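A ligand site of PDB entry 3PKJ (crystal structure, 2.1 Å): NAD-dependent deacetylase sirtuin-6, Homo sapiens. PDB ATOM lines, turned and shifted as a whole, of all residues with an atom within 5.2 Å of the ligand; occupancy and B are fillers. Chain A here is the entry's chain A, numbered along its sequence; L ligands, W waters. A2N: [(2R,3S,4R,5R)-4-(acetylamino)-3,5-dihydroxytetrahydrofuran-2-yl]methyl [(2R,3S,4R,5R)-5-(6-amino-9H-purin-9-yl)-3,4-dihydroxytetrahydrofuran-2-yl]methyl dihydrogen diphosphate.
N of Ser 216 sits at hydrogen-bond distance from OAK of the ligand.
The side-chain hydroxyl (OG) of Ser 216 sits at hydrogen-bond distance from an oxygen (OAJ) of the ligand, at 2.7 Å.
The backbone NH of Arg 65 sits at hydrogen-bond distance from an oxygen (OAD) of the ligand (2.8 Å).
An oxygen (OAJ) of the ligand is in salt-bridge range of the guanidinium group (NH1) of Arg 65 (2.7 Å).
OAI of the ligand sits at hydrogen-bond distance from ND1 of His 133.
ND2 of Asn 240 is in hydrogen-bond range of O3' of the ligand (2.8 Å).
The backbone NH of Phe 64 is in hydrogen-bond range of an oxygen (OAD) of the ligand (2.8 Å).
The backbone NH (N) of Ala 53 is in hydrogen-bond range of an oxygen (OAE) of the ligand.
OG1 of Thr 215 lies within hydrogen-bond range of OAK of the ligand (2.8 Å).
N1 of the ligand lies within hydrogen-bond range of N of Val 258 (2.9 Å).
An oxygen (O2') of the ligand sits close to the backbone NH (N) of Gln 242.
An oxygen (O3') of the ligand sits at hydrogen-bond distance from the side-chain amide oxygen (OE1) of Gln 242 (3.0 Å).
An oxygen (OAI) of the ligand lies within hydrogen-bond range of the backbone carbonyl oxygen of Gln 113 (3.0 Å).
The side-chain hydroxyl (OG1) of Thr 57 is in hydrogen-bond range of a nitrogen (N7) of the ligand.
OAF of the ligand lies within hydrogen-bond range of NE1 of Trp 71, 3.2 Å away.
The backbone NH (N) of Leu 241 is in hydrogen-bond range of a nitrogen (N3) of the ligand, 3.5 Å away.
The backbone carbonyl oxygen (O) of Arg 65 is in hydrogen-bond range of the side-chain amide nitrogen (NE2) of Gln 242, 3.1 Å away.
The backbone carbonyl oxygen (O) of Gly 214 is in hydrogen-bond range of the backbone NH (N) of Ala 53 (3.4 Å).
N of Ala 53 lies within hydrogen-bond range of OD1 of Asn 114 (2.8 Å).
The backbone NH (N) of Leu 217 lies close to the side-chain hydroxyl (OG1) of Thr 215 (3.4 Å).
The backbone carbonyl oxygen of Gly 54 is in hydrogen-bond range of the side-chain hydroxyl of Thr 57, at 2.8 Å.
The backbone carbonyl oxygen (O) of Gly 214 lies within hydrogen-bond range of the backbone NH (N) of Gly 54 (2.8 Å).
O of Val 239 lies within hydrogen-bond range of N of Gly 214.
The backbone NH (N) of Gly 66 is in hydrogen-bond range of the side-chain carboxylate (OD2) of Asp 63.
O of Gly 54 sits close to N7 of the ligand, at 3.3 Å.
O of Gly 214 lies close to O4' of the ligand (3.1 Å).
Gly 52 touches the ligand.
Asp 63 touches the ligand (OD1 to C8, 3.2 Å).
Leu 186 touches the ligand.
CH2 of Trp 188 touches OAF of the ligand, 3.6 Å away.
CG1 of Ile 219 touches OAV of the ligand, 3.4 Å away.
Gly 256 touches the ligand (O to C2, 3.2 Å).
Tyr 257 touches the ligand.
Hydrophobic or aromatic side chains within 4 Å of the ligand: Ala 53, Phe 64, Trp 71, His 133, Trp 188, Ile 219, Leu 241, Tyr 257 and Val 258.
22 residues have an atom within 4 Å of the ligand: Gly 52, Ala 53, Gly 54, Thr 57, Asp 63, Phe 64, Arg 65, Trp 71, Gln 113, His 133, Leu 186, Trp 188, Gly 214, Thr 215, Ser 216, Ile 219, Asn 240, Leu 241, Gln 242, Gly 256, Tyr 257 and Val 258.
The nearest printed residue that does not touch the ligand is Leu 217 (4.1 Å).
Water W2 bridges a nitrogen (N6) of the ligand (3.0 Å) and the backbone NH (N) of Val 258 (3.2 Å).
Water W3 lies within hydrogen-bond range of the side-chain hydroxyl (OG) of Ser 216 (3.0 Å), the backbone NH (N) of Ile 219 (3.1 Å), an oxygen (OAK) of the ligand (3.3 Å) and the backbone NH (N) of Leu 217 (3.4 Å).
Water W4 lies within hydrogen-bond range of O of Gly 54 (2.7 Å), OG1 of Thr 57 (3.1 Å) and N6 of the ligand (3.4 Å).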
ATOM      1  N   GLU A  22     -21.012 -15.070  -3.795  1.00  0.00           N
ATOM      2  CA  GLU A  22     -20.679 -15.864  -4.974  1.00  0.00           C
ATOM      3  C   GLU A  22     -19.659 -15.151  -5.849  1.00  0.00           C
ATOM      4  O   GLU A  22     -19.764 -13.934  -6.050  1.00  0.00           O
ATOM      5  CB  GLU A  22     -21.938 -16.193  -5.791  1.00  0.00           C
ATOM      6  CG  GLU A  22     -22.868 -17.193  -5.108  1.00  0.00           C
ATOM      7  CD  GLU A  22     -24.013 -17.694  -5.980  1.00  0.00           C
ATOM      8  OE1 GLU A  22     -24.574 -16.879  -6.750  1.00  0.00           O
ATOM      9  OE2 GLU A  22     -24.350 -18.895  -5.868  1.00  0.00           O
ATOM     10  N   THR A  51     -18.729 -34.794  -5.929  1.00  0.00           N
ATOM     11  CA  THR A  51     -19.902 -33.958  -6.133  1.00  0.00           C
ATOM     12  C   THR A  51     -20.643 -33.613  -4.851  1.00  0.00           C
ATOM     13  O   THR A  51     -20.696 -34.407  -3.911  1.00  0.00           O
ATOM     14  CB  THR A  51     -20.853 -34.571  -7.164  1.00  0.00           C
ATOM     15  OG1 THR A  51     -21.305 -35.844  -6.702  1.00  0.00           O
ATOM     16  CG2 THR A  51     -20.218 -34.695  -8.553  1.00  0.00           C
ATOM     17  N   GLY A  52     -21.225 -32.428  -4.847  1.00  0.00           N
ATOM     18  CA  GLY A  52     -22.012 -31.891  -3.756  1.00  0.00           C
ATOM     19  C   GLY A  52     -23.352 -31.372  -4.223  1.00  0.00           C
ATOM     20  O   GLY A  52     -23.702 -31.528  -5.406  1.00  0.00           O
ATOM     21  N   ALA A  53     -24.126 -30.769  -3.298  1.00  0.00           N
ATOM     22  CA  ALA A  53     -25.493 -30.256  -3.498  1.00  0.00           C
ATOM     23  C   ALA A  53     -25.663 -29.248  -4.668  1.00  0.00           C
ATOM     24  O   ALA A  53     -26.763 -29.139  -5.212  1.00  0.00           O
ATOM     25  CB  ALA A  53     -26.020 -29.659  -2.198  1.00  0.00           C
ATOM     26  N   GLY A  54     -24.587 -28.556  -5.026  1.00  0.00           N
ATOM     27  CA  GLY A  54     -24.575 -27.582  -6.105  1.00  0.00           C
ATOM     28  C   GLY A  54     -24.827 -28.124  -7.500  1.00  0.00           C
ATOM     29  O   GLY A  54     -25.363 -27.391  -8.337  1.00  0.00           O
ATOM     30  N   ILE A  55     -24.477 -29.391  -7.784  1.00  0.00           N
ATOM     31  CA  ILE A  55     -24.711 -29.979  -9.124  1.00  0.00           C
ATOM     32  C   ILE A  55     -26.213 -30.395  -9.322  1.00  0.00           C
ATOM     33  O   ILE A  55     -26.561 -30.925 -10.370  1.00  0.00           O
ATOM     34  CB  ILE A  55     -23.736 -31.141  -9.506  1.00  0.00           C
ATOM     35  CG1 ILE A  55     -24.003 -32.425  -8.677  1.00  0.00           C
ATOM     36  CG2 ILE A  55     -22.285 -30.720  -9.385  1.00  0.00           C
ATOM     37  CD1 ILE A  55     -23.746 -33.711  -9.459  1.00  0.00           C
ATOM     38  N   THR A  57     -28.827 -28.039  -8.134  1.00  0.00           N
ATOM     39  CA  THR A  57     -29.551 -26.770  -8.067  1.00  0.00           C
ATOM     40  C   THR A  57     -30.200 -26.395  -9.406  1.00  0.00           C
ATOM     41  O   THR A  57     -31.285 -25.808  -9.415  1.00  0.00           O
ATOM     42  CB  THR A  57     -28.667 -25.644  -7.520  1.00  0.00           C
ATOM     43  OG1 THR A  57     -27.506 -25.518  -8.335  1.00  0.00           O
ATOM     44  CG2 THR A  57     -28.272 -25.866  -6.048  1.00  0.00           C
ATOM     45  N   ASP A  63     -29.249 -26.074  -2.553  1.00  0.00           N
ATOM     46  CA  ASP A  63     -28.061 -26.554  -1.837  1.00  0.00           C
ATOM     47  C   ASP A  63     -28.233 -26.299  -0.324  1.00  0.00           C
ATOM     48  O   ASP A  63     -29.347 -26.037   0.117  1.00  0.00           O
ATOM     49  CB  ASP A  63     -26.753 -25.950  -2.428  1.00  0.00           C
ATOM     50  CG  ASP A  63     -26.644 -24.433  -2.445  1.00  0.00           C
ATOM     51  OD1 ASP A  63     -25.810 -23.915  -3.203  1.00  0.00           O
ATOM     52  OD2 ASP A  63     -27.388 -23.768  -1.701  1.00  0.00           O
ATOM     53  N   PHE A  64     -27.156 -26.382   0.468  1.00  0.00           N
ATOM     54  CA  PHE A  64     -27.253 -26.190   1.912  1.00  0.00           C
ATOM     55  C   PHE A  64     -26.727 -24.833   2.384  1.00  0.00           C
ATOM     56  O   PHE A  64     -27.343 -24.218   3.262  1.00  0.00           O
ATOM     57  CB  PHE A  64     -26.532 -27.329   2.652  1.00  0.00           C
ATOM     58  CG  PHE A  64     -27.180 -28.680   2.470  1.00  0.00           C
ATOM     59  CD1 PHE A  64     -26.792 -29.535   1.438  1.00  0.00           C
ATOM     60  CD2 PHE A  64     -28.193 -29.120   3.332  1.00  0.00           C
ATOM     61  CE1 PHE A  64     -27.397 -30.775   1.266  1.00  0.00           C
ATOM     62  CE2 PHE A  64     -28.792 -30.364   3.149  1.00  0.00           C
ATOM     63  CZ  PHE A  64     -28.386 -31.187   2.124  1.00  0.00           C
ATOM     64  N   ARG A  65     -25.580 -24.373   1.826  1.00  0.00           N
ATOM     65  CA  ARG A  65     -24.901 -23.153   2.270  1.00  0.00           C
ATOM     66  C   ARG A  65     -24.823 -22.039   1.197  1.00  0.00           C
ATOM     67  O   ARG A  65     -24.180 -21.010   1.438  1.00  0.00           O
ATOM     68  CB  ARG A  65     -23.491 -23.508   2.787  1.00  0.00           C
ATOM     69  CG  ARG A  65     -23.543 -24.450   4.012  1.00  0.00           C
ATOM     70  CD  ARG A  65     -22.221 -25.079   4.378  1.00  0.00           C
ATOM     71  NE  ARG A  65     -22.412 -26.085   5.428  1.00  0.00           N
ATOM     72  CZ  ARG A  65     -22.621 -27.381   5.209  1.00  0.00           C
ATOM     73  NH1 ARG A  65     -22.638 -27.863   3.973  1.00  0.00           N
ATOM     74  NH2 ARG A  65     -22.811 -28.208   6.225  1.00  0.00           N
ATOM     75  N   GLY A  66     -25.527 -22.213   0.079  1.00  0.00           N
ATOM     76  CA  GLY A  66     -25.585 -21.219  -0.989  1.00  0.00           C
ATOM     77  C   GLY A  66     -26.434 -20.013  -0.607  1.00  0.00           C
ATOM     78  O   GLY A  66     -27.104 -20.057   0.429  1.00  0.00           O
ATOM     79  N   TRP A  71     -29.691 -24.330   5.014  1.00  0.00           N
ATOM     80  CA  TRP A  71     -29.238 -23.778   6.286  1.00  0.00           C
ATOM     81  C   TRP A  71     -29.121 -22.243   6.249  1.00  0.00           C
ATOM     82  O   TRP A  71     -29.282 -21.621   7.303  1.00  0.00           O
ATOM     83  CB  TRP A  71     -27.936 -24.438   6.757  1.00  0.00           C
ATOM     84  CG  TRP A  71     -27.952 -25.949   6.847  1.00  0.00           C
ATOM     85  CD1 TRP A  71     -26.958 -26.798   6.453  1.00  0.00           C
ATOM     86  CD2 TRP A  71     -28.996 -26.785   7.395  1.00  0.00           C
ATOM     87  NE1 TRP A  71     -27.305 -28.105   6.714  1.00  0.00           N
ATOM     88  CE2 TRP A  71     -28.550 -28.123   7.285  1.00  0.00           C
ATOM     89  CE3 TRP A  71     -30.258 -26.530   7.973  1.00  0.00           C
ATOM     90  CZ2 TRP A  71     -29.330 -29.215   7.728  1.00  0.00           C
ATOM     91  CZ3 TRP A  71     -31.026 -27.610   8.402  1.00  0.00           C
ATOM     92  CH2 TRP A  71     -30.563 -28.926   8.268  1.00  0.00           C
ATOM     93  N   GLN A 113     -21.657 -36.619  -1.957  1.00  0.00           N
ATOM     94  CA  GLN A 113     -22.224 -36.220  -0.667  1.00  0.00           C
ATOM     95  C   GLN A 113     -23.750 -36.083  -0.778  1.00  0.00           C
ATOM     96  O   GLN A 113     -24.436 -35.945   0.241  1.00  0.00           O
ATOM     97  CB  GLN A 113     -21.605 -34.882  -0.226  1.00  0.00           C
ATOM     98  CG  GLN A 113     -20.114 -34.978   0.092  1.00  0.00           C
ATOM     99  CD  GLN A 113     -19.519 -33.645   0.458  1.00  0.00           C
ATOM    100  OE1 GLN A 113     -19.756 -33.094   1.527  1.00  0.00           O
ATOM    101  NE2 GLN A 113     -18.687 -33.121  -0.418  1.00  0.00           N
ATOM    102  N   ASN A 114     -24.275 -36.128  -2.017  1.00  0.00           N
ATOM    103  CA  ASN A 114     -25.693 -35.972  -2.340  1.00  0.00           C
ATOM    104  C   ASN A 114     -26.565 -37.164  -1.977  1.00  0.00           C
ATOM    105  O   ASN A 114     -26.193 -38.312  -2.241  1.00  0.00           O
ATOM    106  CB  ASN A 114     -25.850 -35.641  -3.828  1.00  0.00           C
ATOM    107  CG  ASN A 114     -25.246 -34.308  -4.185  1.00  0.00           C
ATOM    108  OD1 ASN A 114     -25.105 -33.434  -3.329  1.00  0.00           O
ATOM    109  ND2 ASN A 114     -24.872 -34.119  -5.454  1.00  0.00           N
ATOM    110  N   HIS A 133     -23.238 -39.876   2.224  1.00  0.00           N
ATOM    111  CA  HIS A 133     -24.288 -39.440   3.145  1.00  0.00           C
ATOM    112  C   HIS A 133     -25.601 -40.227   2.927  1.00  0.00           C
ATOM    113  O   HIS A 133     -26.597 -39.970   3.602  1.00  0.00           O
ATOM    114  CB  HIS A 133     -24.497 -37.920   3.025  1.00  0.00           C
ATOM    115  CG  HIS A 133     -23.254 -37.122   3.318  1.00  0.00           C
ATOM    116  ND1 HIS A 133     -23.080 -35.849   2.804  1.00  0.00           N
ATOM    117  CD2 HIS A 133     -22.153 -37.454   4.036  1.00  0.00           C
ATOM    118  CE1 HIS A 133     -21.902 -35.440   3.250  1.00  0.00           C
ATOM    119  NE2 HIS A 133     -21.301 -36.373   3.985  1.00  0.00           N
ATOM    120  N   LEU A 186     -27.926 -40.558   6.612  1.00  0.00           N
ATOM    121  CA  LEU A 186     -27.207 -40.389   7.872  1.00  0.00           C
ATOM    122  C   LEU A 186     -27.610 -39.103   8.546  1.00  0.00           C
ATOM    123  O   LEU A 186     -27.659 -38.051   7.899  1.00  0.00           O
ATOM    124  CB  LEU A 186     -25.682 -40.390   7.667  1.00  0.00           C
ATOM    125  CG  LEU A 186     -25.038 -41.615   7.024  1.00  0.00           C
ATOM    126  CD1 LEU A 186     -23.600 -41.352   6.750  1.00  0.00           C
ATOM    127  CD2 LEU A 186     -25.176 -42.854   7.907  1.00  0.00           C
ATOM    128  N   TRP A 188     -26.790 -36.160  11.632  1.00  0.00           N
ATOM    129  CA  TRP A 188     -25.555 -35.458  11.992  1.00  0.00           C
ATOM    130  C   TRP A 188     -24.620 -36.306  12.867  1.00  0.00           C
ATOM    131  O   TRP A 188     -23.400 -36.256  12.679  1.00  0.00           O
ATOM    132  CB  TRP A 188     -25.889 -34.136  12.685  1.00  0.00           C
ATOM    133  CG  TRP A 188     -26.417 -33.084  11.748  1.00  0.00           C
ATOM    134  CD1 TRP A 188     -27.716 -32.691  11.593  1.00  0.00           C
ATOM    135  CD2 TRP A 188     -25.648 -32.307  10.824  1.00  0.00           C
ATOM    136  NE1 TRP A 188     -27.805 -31.717  10.636  1.00  0.00           N
ATOM    137  CE2 TRP A 188     -26.547 -31.450  10.143  1.00  0.00           C
ATOM    138  CE3 TRP A 188     -24.287 -32.252  10.486  1.00  0.00           C
ATOM    139  CZ2 TRP A 188     -26.132 -30.538   9.164  1.00  0.00           C
ATOM    140  CZ3 TRP A 188     -23.862 -31.353   9.518  1.00  0.00           C
ATOM    141  CH2 TRP A 188     -24.776 -30.510   8.869  1.00  0.00           C
ATOM    142  N   GLY A 214     -19.660 -28.480  -7.366  1.00  0.00           N
ATOM    143  CA  GLY A 214     -20.778 -28.022  -6.521  1.00  0.00           C
ATOM    144  C   GLY A 214     -20.746 -28.401  -5.057  1.00  0.00           C
ATOM    145  O   GLY A 214     -21.808 -28.628  -4.449  1.00  0.00           O
ATOM    146  N   THR A 215     -19.537 -28.449  -4.442  1.00  0.00           N
ATOM    147  CA  THR A 215     -19.396 -28.754  -3.018  1.00  0.00           C
ATOM    148  C   THR A 215     -18.553 -27.685  -2.307  1.00  0.00           C
ATOM    149  O   THR A 215     -17.519 -27.269  -2.840  1.00  0.00           O
ATOM    150  CB  THR A 215     -18.885 -30.196  -2.756  1.00  0.00           C
ATOM    151  OG1 THR A 215     -18.765 -30.410  -1.345  1.00  0.00           O
ATOM    152  CG2 THR A 215     -17.575 -30.528  -3.468  1.00  0.00           C
ATOM    153  N   SER A 216     -19.012 -27.235  -1.119  1.00  0.00           N
ATOM    154  CA  SER A 216     -18.319 -26.235  -0.309  1.00  0.00           C
ATOM    155  C   SER A 216     -17.111 -26.852   0.437  1.00  0.00           C
ATOM    156  O   SER A 216     -16.260 -26.101   0.933  1.00  0.00           O
ATOM    157  CB  SER A 216     -19.283 -25.598   0.694  1.00  0.00           C
ATOM    158  OG  SER A 216     -19.686 -26.516   1.691  1.00  0.00           O
ATOM    159  N   LEU A 217     -17.057 -28.214   0.522  1.00  0.00           N
ATOM    160  CA  LEU A 217     -16.008 -29.031   1.159  1.00  0.00           C
ATOM    161  C   LEU A 217     -15.821 -28.707   2.668  1.00  0.00           C
ATOM    162  O   LEU A 217     -14.717 -28.851   3.201  1.00  0.00           O
ATOM    163  CB  LEU A 217     -14.647 -28.894   0.403  1.00  0.00           C
ATOM    164  CG  LEU A 217     -14.630 -29.320  -1.079  1.00  0.00           C
ATOM    165  CD1 LEU A 217     -13.466 -28.671  -1.796  1.00  0.00           C
ATOM    166  CD2 LEU A 217     -14.565 -30.830  -1.219  1.00  0.00           C
ATOM    167  N   ILE A 219     -17.811 -30.209   5.215  1.00  0.00           N
ATOM    168  CA  ILE A 219     -18.138 -31.382   6.033  1.00  0.00           C
ATOM    169  C   ILE A 219     -17.033 -32.439   5.902  1.00  0.00           C
ATOM    170  O   ILE A 219     -16.740 -32.892   4.796  1.00  0.00           O
ATOM    171  CB  ILE A 219     -19.568 -31.941   5.690  1.00  0.00           C
ATOM    172  CG1 ILE A 219     -20.686 -30.934   6.112  1.00  0.00           C
ATOM    173  CG2 ILE A 219     -19.820 -33.337   6.299  1.00  0.00           C
ATOM    174  CD1 ILE A 219     -20.784 -30.545   7.690  1.00  0.00           C
ATOM    175  N   VAL A 239     -14.424 -26.627  -8.663  1.00  0.00           N
ATOM    176  CA  VAL A 239     -15.443 -25.918  -9.441  1.00  0.00           C
ATOM    177  C   VAL A 239     -16.591 -25.606  -8.462  1.00  0.00           C
ATOM    178  O   VAL A 239     -17.293 -26.516  -7.988  1.00  0.00           O
ATOM    179  CB  VAL A 239     -15.922 -26.727 -10.681  1.00  0.00           C
ATOM    180  CG1 VAL A 239     -16.903 -25.917 -11.510  1.00  0.00           C
ATOM    181  CG2 VAL A 239     -14.738 -27.174 -11.551  1.00  0.00           C
ATOM    182  N   ASN A 240     -16.743 -24.308  -8.111  1.00  0.00           N
ATOM    183  CA  ASN A 240     -17.766 -23.830  -7.179  1.00  0.00           C
ATOM    184  C   ASN A 240     -18.017 -22.343  -7.357  1.00  0.00           C
ATOM    185  O   ASN A 240     -17.079 -21.602  -7.662  1.00  0.00           O
ATOM    186  CB  ASN A 240     -17.334 -24.106  -5.733  1.00  0.00           C
ATOM    187  CG  ASN A 240     -18.472 -24.379  -4.795  1.00  0.00           C
ATOM    188  OD1 ASN A 240     -19.285 -25.281  -5.024  1.00  0.00           O
ATOM    189  ND2 ASN A 240     -18.541 -23.646  -3.700  1.00  0.00           N
ATOM    190  N   LEU A 241     -19.260 -21.898  -7.137  1.00  0.00           N
ATOM    191  CA  LEU A 241     -19.631 -20.478  -7.223  1.00  0.00           C
ATOM    192  C   LEU A 241     -19.098 -19.714  -5.993  1.00  0.00           C
ATOM    193  O   LEU A 241     -18.502 -18.645  -6.147  1.00  0.00           O
ATOM    194  CB  LEU A 241     -21.161 -20.311  -7.348  1.00  0.00           C
ATOM    195  CG  LEU A 241     -21.807 -20.673  -8.691  1.00  0.00           C
ATOM    196  CD1 LEU A 241     -23.305 -20.790  -8.545  1.00  0.00           C
ATOM    197  CD2 LEU A 241     -21.477 -19.655  -9.754  1.00  0.00           C
ATOM    198  N   GLN A 242     -19.295 -20.278  -4.794  1.00  0.00           N
ATOM    199  CA  GLN A 242     -18.846 -19.736  -3.512  1.00  0.00           C
ATOM    200  C   GLN A 242     -17.418 -20.211  -3.192  1.00  0.00           C
ATOM    201  O   GLN A 242     -16.979 -21.221  -3.774  1.00  0.00           O
ATOM    202  CB  GLN A 242     -19.774 -20.207  -2.384  1.00  0.00           C
ATOM    203  CG  GLN A 242     -21.087 -19.425  -2.250  1.00  0.00           C
ATOM    204  CD  GLN A 242     -21.955 -19.969  -1.136  1.00  0.00           C
ATOM    205  OE1 GLN A 242     -21.860 -21.136  -0.740  1.00  0.00           O
ATOM    206  NE2 GLN A 242     -22.841 -19.143  -0.630  1.00  0.00           N
ATOM    207  N   PRO A 243     -16.675 -19.566  -2.232  1.00  0.00           N
ATOM    208  CA  PRO A 243     -15.345 -20.082  -1.878  1.00  0.00           C
ATOM    209  C   PRO A 243     -15.455 -21.405  -1.104  1.00  0.00           C
ATOM    210  O   PRO A 243     -16.480 -21.642  -0.450  1.00  0.00           O
ATOM    211  CB  PRO A 243     -14.743 -18.971  -1.001  1.00  0.00           C
ATOM    212  CG  PRO A 243     -15.672 -17.811  -1.108  1.00  0.00           C
ATOM    213  CD  PRO A 243     -17.012 -18.382  -1.417  1.00  0.00           C
ATOM    214  N   GLY A 256     -17.892 -20.607 -11.490  1.00  0.00           N
ATOM    215  CA  GLY A 256     -18.996 -20.586 -12.442  1.00  0.00           C
ATOM    216  C   GLY A 256     -19.995 -21.705 -12.222  1.00  0.00           C
ATOM    217  O   GLY A 256     -19.822 -22.524 -11.307  1.00  0.00           O
ATOM    218  N   TYR A 257     -21.061 -21.734 -13.034  1.00  0.00           N
ATOM    219  CA  TYR A 257     -22.094 -22.766 -12.947  1.00  0.00           C
ATOM    220  C   TYR A 257     -21.525 -24.078 -13.490  1.00  0.00           C
ATOM    221  O   TYR A 257     -20.944 -24.094 -14.576  1.00  0.00           O
ATOM    222  CB  TYR A 257     -23.362 -22.343 -13.718  1.00  0.00           C
ATOM    223  CG  TYR A 257     -24.030 -21.122 -13.149  1.00  0.00           C
ATOM    224  CD1 TYR A 257     -24.867 -21.220 -12.038  1.00  0.00           C
ATOM    225  CD2 TYR A 257     -23.842 -19.863 -13.710  1.00  0.00           C
ATOM    226  CE1 TYR A 257     -25.503 -20.097 -11.508  1.00  0.00           C
ATOM    227  CE2 TYR A 257     -24.465 -18.729 -13.195  1.00  0.00           C
ATOM    228  CZ  TYR A 257     -25.296 -18.854 -12.086  1.00  0.00           C
ATOM    229  OH  TYR A 257     -25.920 -17.742 -11.563  1.00  0.00           O
ATOM    230  N   VAL A 258     -21.680 -25.170 -12.718  1.00  0.00           N
ATOM    231  CA  VAL A 258     -21.162 -26.509 -13.053  1.00  0.00           C
ATOM    232  C   VAL A 258     -21.650 -26.992 -14.426  1.00  0.00           C
ATOM    233  O   VAL A 258     -20.849 -27.587 -15.152  1.00  0.00           O
ATOM    234  CB  VAL A 258     -21.364 -27.582 -11.950  1.00  0.00           C
ATOM    235  CG1 VAL A 258     -20.389 -27.414 -10.801  1.00  0.00           C
ATOM    236  CG2 VAL A 258     -22.803 -27.672 -11.463  1.00  0.00           C
HETATM  237  N1  A2N L   1     -22.545 -24.436 -10.050  1.00  0.00           N
HETATM  238  C2  A2N L   1     -21.468 -24.429  -9.275  1.00  0.00           C
HETATM  239  N3  A2N L   1     -21.574 -24.372  -7.952  1.00  0.00           N
HETATM  240  C4  A2N L   1     -22.784 -24.324  -7.366  1.00  0.00           C
HETATM  241  C5  A2N L   1     -23.924 -24.316  -8.142  1.00  0.00           C
HETATM  242  C6  A2N L   1     -23.790 -24.375  -9.527  1.00  0.00           C
HETATM  243  N6  A2N L   1     -24.855 -24.369 -10.316  1.00  0.00           N
HETATM  244  N7  A2N L   1     -24.968 -24.240  -7.323  1.00  0.00           N
HETATM  245  C8  A2N L   1     -24.496 -24.193  -6.073  1.00  0.00           C
HETATM  246  N9  A2N L   1     -23.163 -24.229  -6.104  1.00  0.00           N
HETATM  247  C1' A2N L   1     -22.246 -24.287  -4.949  1.00  0.00           C
HETATM  248  C2' A2N L   1     -22.647 -23.389  -3.800  1.00  0.00           C
HETATM  249  O2' A2N L   1     -21.975 -22.151  -3.938  1.00  0.00           O
HETATM  250  C3' A2N L   1     -22.123 -24.160  -2.571  1.00  0.00           C
HETATM  251  O3' A2N L   1     -20.875 -23.625  -2.121  1.00  0.00           O
HETATM  252  C4' A2N L   1     -21.874 -25.584  -3.103  1.00  0.00           C
HETATM  253  O4' A2N L   1     -22.401 -25.614  -4.428  1.00  0.00           O
HETATM  254  C5' A2N L   1     -22.698 -26.571  -2.316  1.00  0.00           C
HETATM  255  O5' A2N L   1     -22.167 -26.720  -1.015  1.00  0.00           O
HETATM  256  CAA A2N L   1     -27.597 -33.756   5.343  1.00  0.00           C
HETATM  257  OAC A2N L   1     -25.995 -35.457   5.885  1.00  0.00           O
HETATM  258  OAD A2N L   1     -24.369 -26.149   0.084  1.00  0.00           O
HETATM  259  OAE A2N L   1     -22.777 -30.857  -0.809  1.00  0.00           O
HETATM  260  OAF A2N L   1     -25.393 -30.201   5.312  1.00  0.00           O
HETATM  261  OAI A2N L   1     -24.657 -33.653   2.183  1.00  0.00           O
HETATM  262  OAJ A2N L   1     -22.332 -26.822   1.508  1.00  0.00           O
HETATM  263  OAK A2N L   1     -20.993 -29.142  -0.128  1.00  0.00           O
HETATM  264  CAO A2N L   1     -22.406 -31.624   1.989  1.00  0.00           C
HETATM  265  NAS A2N L   1     -25.213 -33.671   4.781  1.00  0.00           N
HETATM  266  OAU A2N L   1     -22.488 -30.234   1.657  1.00  0.00           O
HETATM  267  OAV A2N L   1     -23.471 -30.906   4.109  1.00  0.00           O
HETATM  268  OAX A2N L   1     -23.545 -28.566   0.039  1.00  0.00           O
HETATM  269  CAY A2N L   1     -26.191 -34.364   5.359  1.00  0.00           C
HETATM  270  CBC A2N L   1     -24.588 -31.325   4.959  1.00  0.00           C
HETATM  271  CBF A2N L   1     -24.662 -32.354   2.784  1.00  0.00           C
HETATM  272  CBH A2N L   1     -23.246 -31.997   3.215  1.00  0.00           C
HETATM  273  CBI A2N L   1     -25.386 -32.356   4.131  1.00  0.00           C
HETATM  274  PBL A2N L   1     -23.166 -26.996   0.179  1.00  0.00           P
HETATM  275  PBM A2N L   1     -22.450 -29.757   0.111  1.00  0.00           P
HETATM  276  O   HOH W   1     -23.696 -35.882   8.141  1.00  0.00           O
HETATM  277  O   HOH W   2     -24.772 -25.707 -13.002  1.00  0.00           O
HETATM  278  O   HOH W   3     -19.429 -29.248   2.782  1.00  0.00           O
HETATM  279  O   HOH W   4     -26.583 -27.213 -10.701  1.00  0.00           O
